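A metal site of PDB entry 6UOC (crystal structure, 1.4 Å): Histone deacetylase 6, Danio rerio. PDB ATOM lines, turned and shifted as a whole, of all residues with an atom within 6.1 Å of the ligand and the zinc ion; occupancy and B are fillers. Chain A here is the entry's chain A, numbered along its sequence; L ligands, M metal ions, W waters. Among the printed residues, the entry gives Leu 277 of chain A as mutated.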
ATOM      1  N   SER A  28     -29.884  19.313 -21.536  1.00  0.00           N
ATOM      2  CA  SER A  28     -29.052  18.126 -21.624  1.00  0.00           C
ATOM      3  C   SER A  28     -29.237  17.174 -20.444  1.00  0.00           C
ATOM      4  O   SER A  28     -28.516  16.179 -20.348  1.00  0.00           O
ATOM      5  CB  SER A  28     -27.575  18.515 -21.702  1.00  0.00           C
ATOM      6  OG  SER A  28     -27.127  19.038 -20.468  1.00  0.00           O
ATOM      7  N   ASP A  96     -30.202  17.658  -3.281  1.00  0.00           N
ATOM      8  CA  ASP A  96     -29.047  17.250  -4.063  1.00  0.00           C
ATOM      9  C   ASP A  96     -29.500  16.518  -5.322  1.00  0.00           C
ATOM     10  O   ASP A  96     -30.248  15.538  -5.242  1.00  0.00           O
ATOM     11  CB  ASP A  96     -28.074  16.382  -3.265  1.00  0.00           C
ATOM     12  CG  ASP A  96     -26.761  16.221  -3.989  1.00  0.00           C
ATOM     13  OD1 ASP A  96     -26.393  15.085  -4.309  1.00  0.00           O
ATOM     14  OD2 ASP A  96     -26.114  17.239  -4.316  1.00  0.00           O
ATOM     15  N   SER A  97     -29.057  17.015  -6.472  1.00  0.00           N
ATOM     16  CA  SER A  97     -29.251  16.350  -7.755  1.00  0.00           C
ATOM     17  C   SER A  97     -30.725  16.189  -8.100  1.00  0.00           C
ATOM     18  O   SER A  97     -31.202  15.091  -8.383  1.00  0.00           O
ATOM     19  CB  SER A  97     -28.535  14.994  -7.812  1.00  0.00           C
ATOM     20  OG  SER A  97     -27.138  15.147  -7.868  1.00  0.00           O
ATOM     21  N   PRO A 137     -38.020   8.318 -11.148  1.00  0.00           N
ATOM     22  CA  PRO A 137     -37.530   7.198 -10.330  1.00  0.00           C
ATOM     23  C   PRO A 137     -37.780   7.467  -8.862  1.00  0.00           C
ATOM     24  O   PRO A 137     -38.242   8.548  -8.464  1.00  0.00           O
ATOM     25  CB  PRO A 137     -36.032   7.177 -10.668  1.00  0.00           C
ATOM     26  CG  PRO A 137     -35.712   8.624 -10.971  1.00  0.00           C
ATOM     27  CD  PRO A 137     -36.925   9.116 -11.729  1.00  0.00           C
ATOM     28  N   HIS A 139     -35.707   5.508  -5.918  1.00  0.00           N
ATOM     29  CA  HIS A 139     -34.942   4.855  -4.861  1.00  0.00           C
ATOM     30  C   HIS A 139     -34.112   5.794  -3.997  1.00  0.00           C
ATOM     31  O   HIS A 139     -33.716   5.389  -2.897  1.00  0.00           O
ATOM     32  CB  HIS A 139     -34.155   3.627  -5.355  1.00  0.00           C
ATOM     33  CG  HIS A 139     -33.001   3.936  -6.256  1.00  0.00           C
ATOM     34  ND1 HIS A 139     -31.889   3.126  -6.299  1.00  0.00           N
ATOM     35  CD2 HIS A 139     -32.789   4.924  -7.165  1.00  0.00           C
ATOM     36  CE1 HIS A 139     -31.029   3.595  -7.190  1.00  0.00           C
ATOM     37  NE2 HIS A 139     -31.551   4.680  -7.731  1.00  0.00           N
ATOM     38  N   HIS A 140     -33.857   7.033  -4.446  1.00  0.00           N
ATOM     39  CA  HIS A 140     -33.123   7.989  -3.630  1.00  0.00           C
ATOM     40  C   HIS A 140     -34.027   8.859  -2.752  1.00  0.00           C
ATOM     41  O   HIS A 140     -33.521   9.542  -1.855  1.00  0.00           O
ATOM     42  CB  HIS A 140     -32.291   8.923  -4.515  1.00  0.00           C
ATOM     43  CG  HIS A 140     -31.269   8.222  -5.339  1.00  0.00           C
ATOM     44  ND1 HIS A 140     -30.290   7.416  -4.795  1.00  0.00           N
ATOM     45  CD2 HIS A 140     -31.088   8.176  -6.684  1.00  0.00           C
ATOM     46  CE1 HIS A 140     -29.542   6.910  -5.755  1.00  0.00           C
ATOM     47  NE2 HIS A 140     -30.000   7.355  -6.907  1.00  0.00           N
ATOM     48  N   GLY A 148     -31.595  12.963  -5.933  1.00  0.00           N
ATOM     49  CA  GLY A 148     -31.199  12.086  -7.024  1.00  0.00           C
ATOM     50  C   GLY A 148     -32.271  11.797  -8.058  1.00  0.00           C
ATOM     51  O   GLY A 148     -32.503  10.650  -8.439  1.00  0.00           O
ATOM     52  N   PHE A 149     -32.954  12.852  -8.504  1.00  0.00           N
ATOM     53  CA  PHE A 149     -33.957  12.811  -9.566  1.00  0.00           C
ATOM     54  C   PHE A 149     -35.283  12.259  -9.050  1.00  0.00           C
ATOM     55  O   PHE A 149     -36.190  12.047  -9.869  1.00  0.00           O
ATOM     56  CB  PHE A 149     -33.566  12.015 -10.819  1.00  0.00           C
ATOM     57  CG  PHE A 149     -32.184  12.316 -11.369  1.00  0.00           C
ATOM     58  CD1 PHE A 149     -31.550  11.363 -12.164  1.00  0.00           C
ATOM     59  CD2 PHE A 149     -31.525  13.517 -11.125  1.00  0.00           C
ATOM     60  CE1 PHE A 149     -30.296  11.585 -12.693  1.00  0.00           C
ATOM     61  CE2 PHE A 149     -30.248  13.742 -11.659  1.00  0.00           C
ATOM     62  CZ  PHE A 149     -29.643  12.768 -12.441  1.00  0.00           C
ATOM     63  N   ASP A 177     -29.777  -0.960  -9.853  1.00  0.00           N
ATOM     64  CA  ASP A 177     -29.311   0.313 -10.382  1.00  0.00           C
ATOM     65  C   ASP A 177     -27.856   0.506  -9.968  1.00  0.00           C
ATOM     66  O   ASP A 177     -27.428   0.041  -8.913  1.00  0.00           O
ATOM     67  CB  ASP A 177     -30.229   1.395  -9.813  1.00  0.00           C
ATOM     68  CG  ASP A 177     -29.965   2.756 -10.394  1.00  0.00           C
ATOM     69  OD1 ASP A 177     -28.970   3.395 -10.002  1.00  0.00           O
ATOM     70  OD2 ASP A 177     -30.796   3.217 -11.227  1.00  0.00           O
ATOM     71  N   VAL A 178     -27.082   1.211 -10.799  1.00  0.00           N
ATOM     72  CA  VAL A 178     -25.664   1.398 -10.506  1.00  0.00           C
ATOM     73  C   VAL A 178     -25.417   2.275  -9.270  1.00  0.00           C
ATOM     74  O   VAL A 178     -24.306   2.280  -8.722  1.00  0.00           O
ATOM     75  CB  VAL A 178     -24.912   1.933 -11.744  1.00  0.00           C
ATOM     76  CG1 VAL A 178     -25.065   3.434 -11.865  1.00  0.00           C
ATOM     77  CG2 VAL A 178     -23.443   1.522 -11.692  1.00  0.00           C
ATOM     78  N   HIS A 179     -26.423   3.029  -8.829  1.00  0.00           N
ATOM     79  CA  HIS A 179     -26.299   3.881  -7.651  1.00  0.00           C
ATOM     80  C   HIS A 179     -26.912   3.213  -6.431  1.00  0.00           C
ATOM     81  O   HIS A 179     -27.853   2.412  -6.528  1.00  0.00           O
ATOM     82  CB  HIS A 179     -27.018   5.219  -7.885  1.00  0.00           C
ATOM     83  CG  HIS A 179     -26.465   6.001  -9.026  1.00  0.00           C
ATOM     84  ND1 HIS A 179     -27.024   5.973 -10.290  1.00  0.00           N
ATOM     85  CD2 HIS A 179     -25.390   6.819  -9.101  1.00  0.00           C
ATOM     86  CE1 HIS A 179     -26.320   6.753 -11.089  1.00  0.00           C
ATOM     87  NE2 HIS A 179     -25.318   7.269 -10.390  1.00  0.00           N
ATOM     88  N   TRP A 208     -20.924   9.246  -6.817  1.00  0.00           N
ATOM     89  CA  TRP A 208     -22.152   9.746  -6.215  1.00  0.00           C
ATOM     90  C   TRP A 208     -23.028   8.565  -5.753  1.00  0.00           C
ATOM     91  O   TRP A 208     -23.131   7.562  -6.467  1.00  0.00           O
ATOM     92  CB  TRP A 208     -22.894  10.594  -7.269  1.00  0.00           C
ATOM     93  CG  TRP A 208     -24.012  11.396  -6.673  1.00  0.00           C
ATOM     94  CD1 TRP A 208     -23.952  12.697  -6.242  1.00  0.00           C
ATOM     95  CD2 TRP A 208     -25.356  10.950  -6.428  1.00  0.00           C
ATOM     96  NE1 TRP A 208     -25.182  13.080  -5.737  1.00  0.00           N
ATOM     97  CE2 TRP A 208     -26.056  12.022  -5.825  1.00  0.00           C
ATOM     98  CE3 TRP A 208     -26.034   9.738  -6.632  1.00  0.00           C
ATOM     99  CZ2 TRP A 208     -27.400  11.919  -5.444  1.00  0.00           C
ATOM    100  CZ3 TRP A 208     -27.363   9.642  -6.251  1.00  0.00           C
ATOM    101  CH2 TRP A 208     -28.021  10.718  -5.665  1.00  0.00           C
ATOM    102  N   HIS A 210     -21.652   9.401  -2.720  1.00  0.00           N
ATOM    103  CA  HIS A 210     -20.496   9.709  -1.861  1.00  0.00           C
ATOM    104  C   HIS A 210     -20.731   9.459  -0.376  1.00  0.00           C
ATOM    105  O   HIS A 210     -20.226  10.216   0.457  1.00  0.00           O
ATOM    106  CB  HIS A 210     -20.083  11.177  -2.023  1.00  0.00           C
ATOM    107  CG  HIS A 210     -20.000  11.641  -3.435  1.00  0.00           C
ATOM    108  ND1 HIS A 210     -19.058  11.166  -4.326  1.00  0.00           N
ATOM    109  CD2 HIS A 210     -20.742  12.545  -4.129  1.00  0.00           C
ATOM    110  CE1 HIS A 210     -19.230  11.750  -5.499  1.00  0.00           C
ATOM    111  NE2 HIS A 210     -20.243  12.598  -5.408  1.00  0.00           N
ATOM    112  N   GLY A 268     -32.980  -0.218 -12.285  1.00  0.00           N
ATOM    113  CA  GLY A 268     -32.225   0.736 -13.059  1.00  0.00           C
ATOM    114  C   GLY A 268     -31.330   0.033 -14.053  1.00  0.00           C
ATOM    115  O   GLY A 268     -30.955  -1.118 -13.854  1.00  0.00           O
ATOM    116  N   ASP A 270     -28.485   1.760 -15.480  1.00  0.00           N
ATOM    117  CA  ASP A 270     -27.271   2.558 -15.624  1.00  0.00           C
ATOM    118  C   ASP A 270     -26.002   1.756 -15.407  1.00  0.00           C
ATOM    119  O   ASP A 270     -24.919   2.316 -15.593  1.00  0.00           O
ATOM    120  CB  ASP A 270     -27.335   3.868 -14.810  1.00  0.00           C
ATOM    121  CG  ASP A 270     -27.996   3.716 -13.445  1.00  0.00           C
ATOM    122  OD1 ASP A 270     -28.191   2.585 -12.964  1.00  0.00           O
ATOM    123  OD2 ASP A 270     -28.317   4.781 -12.858  1.00  0.00           O
ATOM    124  N   PRO A 276     -24.032   6.706 -19.875  1.00  0.00           N
ATOM    125  CA  PRO A 276     -23.073   7.817 -19.796  1.00  0.00           C
ATOM    126  C   PRO A 276     -22.524   8.078 -18.402  1.00  0.00           C
ATOM    127  O   PRO A 276     -21.522   8.795 -18.280  1.00  0.00           O
ATOM    128  CB  PRO A 276     -23.895   9.018 -20.300  1.00  0.00           C
ATOM    129  CG  PRO A 276     -25.303   8.667 -19.945  1.00  0.00           C
ATOM    130  CD  PRO A 276     -25.387   7.180 -20.194  1.00  0.00           C
ATOM    131  N   LEU A 277     -23.141   7.531 -17.354  1.00  0.00           N
ATOM    132  CA  LEU A 277     -22.754   7.776 -15.967  1.00  0.00           C
ATOM    133  C   LEU A 277     -22.220   6.551 -15.243  1.00  0.00           C
ATOM    134  O   LEU A 277     -21.335   6.682 -14.392  1.00  0.00           O
ATOM    135  CB  LEU A 277     -23.953   8.304 -15.168  1.00  0.00           C
ATOM    136  CG  LEU A 277     -24.460   9.683 -15.548  1.00  0.00           C
ATOM    137  CD1 LEU A 277     -25.797   9.984 -14.876  1.00  0.00           C
ATOM    138  CD2 LEU A 277     -23.427  10.731 -15.161  1.00  0.00           C
ATOM    139  N   GLU A 307     -35.858   2.547 -12.459  1.00  0.00           N
ATOM    140  CA  GLU A 307     -35.140   3.554 -11.693  1.00  0.00           C
ATOM    141  C   GLU A 307     -34.317   4.355 -12.692  1.00  0.00           C
ATOM    142  O   GLU A 307     -34.903   5.022 -13.543  1.00  0.00           O
ATOM    143  CB  GLU A 307     -34.316   2.913 -10.568  1.00  0.00           C
ATOM    144  CG  GLU A 307     -35.196   2.186  -9.533  1.00  0.00           C
ATOM    145  CD  GLU A 307     -35.905   3.115  -8.545  1.00  0.00           C
ATOM    146  OE1 GLU A 307     -36.669   2.568  -7.704  1.00  0.00           O
ATOM    147  OE2 GLU A 307     -35.721   4.345  -8.594  1.00  0.00           O
ATOM    148  N   GLY A 308     -32.986   4.270 -12.638  1.00  0.00           N
ATOM    149  CA  GLY A 308     -32.123   4.996 -13.550  1.00  0.00           C
ATOM    150  C   GLY A 308     -31.811   4.222 -14.827  1.00  0.00           C
ATOM    151  O   GLY A 308     -32.450   3.222 -15.166  1.00  0.00           O
ATOM    152  N   GLY A 309     -30.805   4.723 -15.542  1.00  0.00           N
ATOM    153  CA  GLY A 309     -30.476   4.214 -16.865  1.00  0.00           C
ATOM    154  C   GLY A 309     -30.680   5.319 -17.892  1.00  0.00           C
ATOM    155  O   GLY A 309     -31.809   5.750 -18.113  1.00  0.00           O
ATOM    156  N   TYR A 310     -29.587   5.781 -18.511  1.00  0.00           N
ATOM    157  CA  TYR A 310     -29.604   7.044 -19.270  1.00  0.00           C
ATOM    158  C   TYR A 310     -29.130   6.944 -20.696  1.00  0.00           C
ATOM    159  O   TYR A 310     -29.270   7.923 -21.444  1.00  0.00           O
ATOM    160  CB  TYR A 310     -28.823   8.124 -18.502  1.00  0.00           C
ATOM    161  CG  TYR A 310     -29.395   8.232 -17.120  1.00  0.00           C
ATOM    162  CD1 TYR A 310     -30.629   8.807 -16.914  1.00  0.00           C
ATOM    163  CD2 TYR A 310     -28.753   7.618 -16.048  1.00  0.00           C
ATOM    164  CE1 TYR A 310     -31.203   8.855 -15.655  1.00  0.00           C
ATOM    165  CE2 TYR A 310     -29.312   7.649 -14.794  1.00  0.00           C
ATOM    166  CZ  TYR A 310     -30.524   8.258 -14.599  1.00  0.00           C
ATOM    167  OH  TYR A 310     -31.086   8.280 -13.342  1.00  0.00           O
HETATM  168  C1  LIG L   1     -29.324   7.859 -10.752  1.00  0.00           C
HETATM  169  C2  LIG L   1     -28.683   9.175 -10.508  1.00  0.00           C
HETATM  170  C3  LIG L   1     -28.908   9.991  -9.375  1.00  0.00           C
HETATM  171  C4  LIG L   1     -28.216  11.159  -9.134  1.00  0.00           C
HETATM  172  C5  LIG L   1     -27.218  11.615  -9.994  1.00  0.00           C
HETATM  173  C6  LIG L   1     -25.160  12.902  -9.831  1.00  0.00           C
HETATM  174  C7  LIG L   1     -23.291  14.346  -9.458  1.00  0.00           C
HETATM  175  C8  LIG L   1     -22.804  14.732 -10.825  1.00  0.00           C
HETATM  176  C9  LIG L   1     -22.169  13.792 -11.586  1.00  0.00           C
HETATM  177  C10 LIG L   1     -21.680  14.057 -12.867  1.00  0.00           C
HETATM  178  C11 LIG L   1     -21.804  15.314 -13.438  1.00  0.00           C
HETATM  179  C12 LIG L   1     -21.275  15.545 -14.752  1.00  0.00           C
HETATM  180  C13 LIG L   1     -20.642  14.538 -15.459  1.00  0.00           C
HETATM  181  C14 LIG L   1     -20.069  14.706 -16.816  1.00  0.00           C
HETATM  182  C15 LIG L   1     -19.280  16.243 -18.435  1.00  0.00           C
HETATM  183  C16 LIG L   1     -19.531  17.478 -19.309  1.00  0.00           C
HETATM  184  C17 LIG L   1     -21.753  15.827 -18.112  1.00  0.00           C
HETATM  185  C18 LIG L   1     -22.687  16.969 -17.707  1.00  0.00           C
HETATM  186  C19 LIG L   1     -20.543  13.282 -14.846  1.00  0.00           C
HETATM  187  C20 LIG L   1     -21.030  13.053 -13.612  1.00  0.00           C
HETATM  188  C21 LIG L   1     -22.468  16.309 -12.644  1.00  0.00           C
HETATM  189  C22 LIG L   1     -22.934  16.017 -11.386  1.00  0.00           C
HETATM  190  C23 LIG L   1     -26.979  10.796 -11.099  1.00  0.00           C
HETATM  191  C24 LIG L   1     -27.668   9.636 -11.344  1.00  0.00           C
HETATM  192  N1  LIG L   1     -26.529  12.744  -9.743  1.00  0.00           N
HETATM  193  N2  LIG L   1     -20.391  15.968 -17.448  1.00  0.00           N
HETATM  194  N3  LIG L   1     -29.726   7.164  -9.600  1.00  0.00           N
HETATM  195  O1  LIG L   1     -29.360   7.305 -11.821  1.00  0.00           O
HETATM  196  O2  LIG L   1     -24.640  14.066  -9.383  1.00  0.00           O
HETATM  197  O3  LIG L   1     -24.394  12.048 -10.293  1.00  0.00           O
HETATM  198  O4  LIG L   1     -30.264   5.923  -9.672  1.00  0.00           O
HETATM  199 ZN    ZN M   1     -28.889   5.201 -10.949  1.00  0.00          ZN
HETATM  200  O   HOH W   1     -21.231  10.385 -11.687  1.00  0.00           O
HETATM  201  O   HOH W   2     -23.799   9.432 -11.219  1.00  0.00           O
HETATM  202  O   HOH W   3     -19.738  10.301 -16.348  1.00  0.00           O
HETATM  203  O   HOH W   4     -26.033  17.162  -9.168  1.00  0.00           O
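NE2 of His 140 sits close to N3 of the ligand (2.7 Å). An oxygen (O4) of the ligand sits close to a ring nitrogen (NE2) of His 139, at 2.6 Å. OG of Ser 97 sits at hydrogen-bond distance from N1 of the ligand (3.1 Å). An oxygen (O1) of the ligand sits close to the side-chain hydroxyl (OH) of Tyr 310 (2.5 Å).
N of Gly 308 lies within hydrogen-bond range of OD2 of Asp 177 (2.8 Å). O of Ser 97 is in hydrogen-bond range of N of Phe 149. N of Gly 148 lies within hydrogen-bond range of O of Asp 96 (3.0 Å). A ring nitrogen (NE2) of His 140 lies within hydrogen-bond range of a ring nitrogen (NE2) of His 139, 3.2 Å away. OD1 of Asp 270 sits at hydrogen-bond distance from N of Val 178, at 2.8 Å. N of His 139 is in hydrogen-bond range of OE2 of Glu 307 (2.9 Å). O of Ser 97 is in hydrogen-bond range of N of Gly 148 (3.3 Å). NE1 of Trp 208 is in hydrogen-bond range of OD1 of Asp 96.
Residues that only touch the ligand: Gly 148 (3.8 Å), Phe 149 (3.5 Å), Trp 208 (3.4 Å), Leu 277 (3.7 Å) and Gly 308 (3.99 Å). Hydrophobic or aromatic side chains within 4 Å of the ligand: His 139, His 140, Phe 149, His 179, Trp 208, Leu 277 and Tyr 310. The nearest printed residue that does not touch the ligand is Gly 309 (4.8 Å).
Of the 21 residues printed, 3 come within 4 Å of the zinc ion.
The zinc ion is bound by O4 of the ligand (2.0 Å), OD2 of Asp 270 (2.0 Å), OD1 of Asp 177 (2.0 Å), ND1 of His 179 (2.1 Å) and O1 of the ligand (2.3 Å). The zinc ion has five donor atoms within binding distance. Slightly farther from the zinc ion lies the side-chain carboxylate (OD2) of Asp 177 (2.8 Å).
Water W2 bridges NE2 of His 179 (2.8 Å) and O3 of the ligand (2.8 Å). Water W4 bridges the side-chain hydroxyl of Ser 97 (2.6 Å) and an oxygen (O2) of the ligand (3.4 Å).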
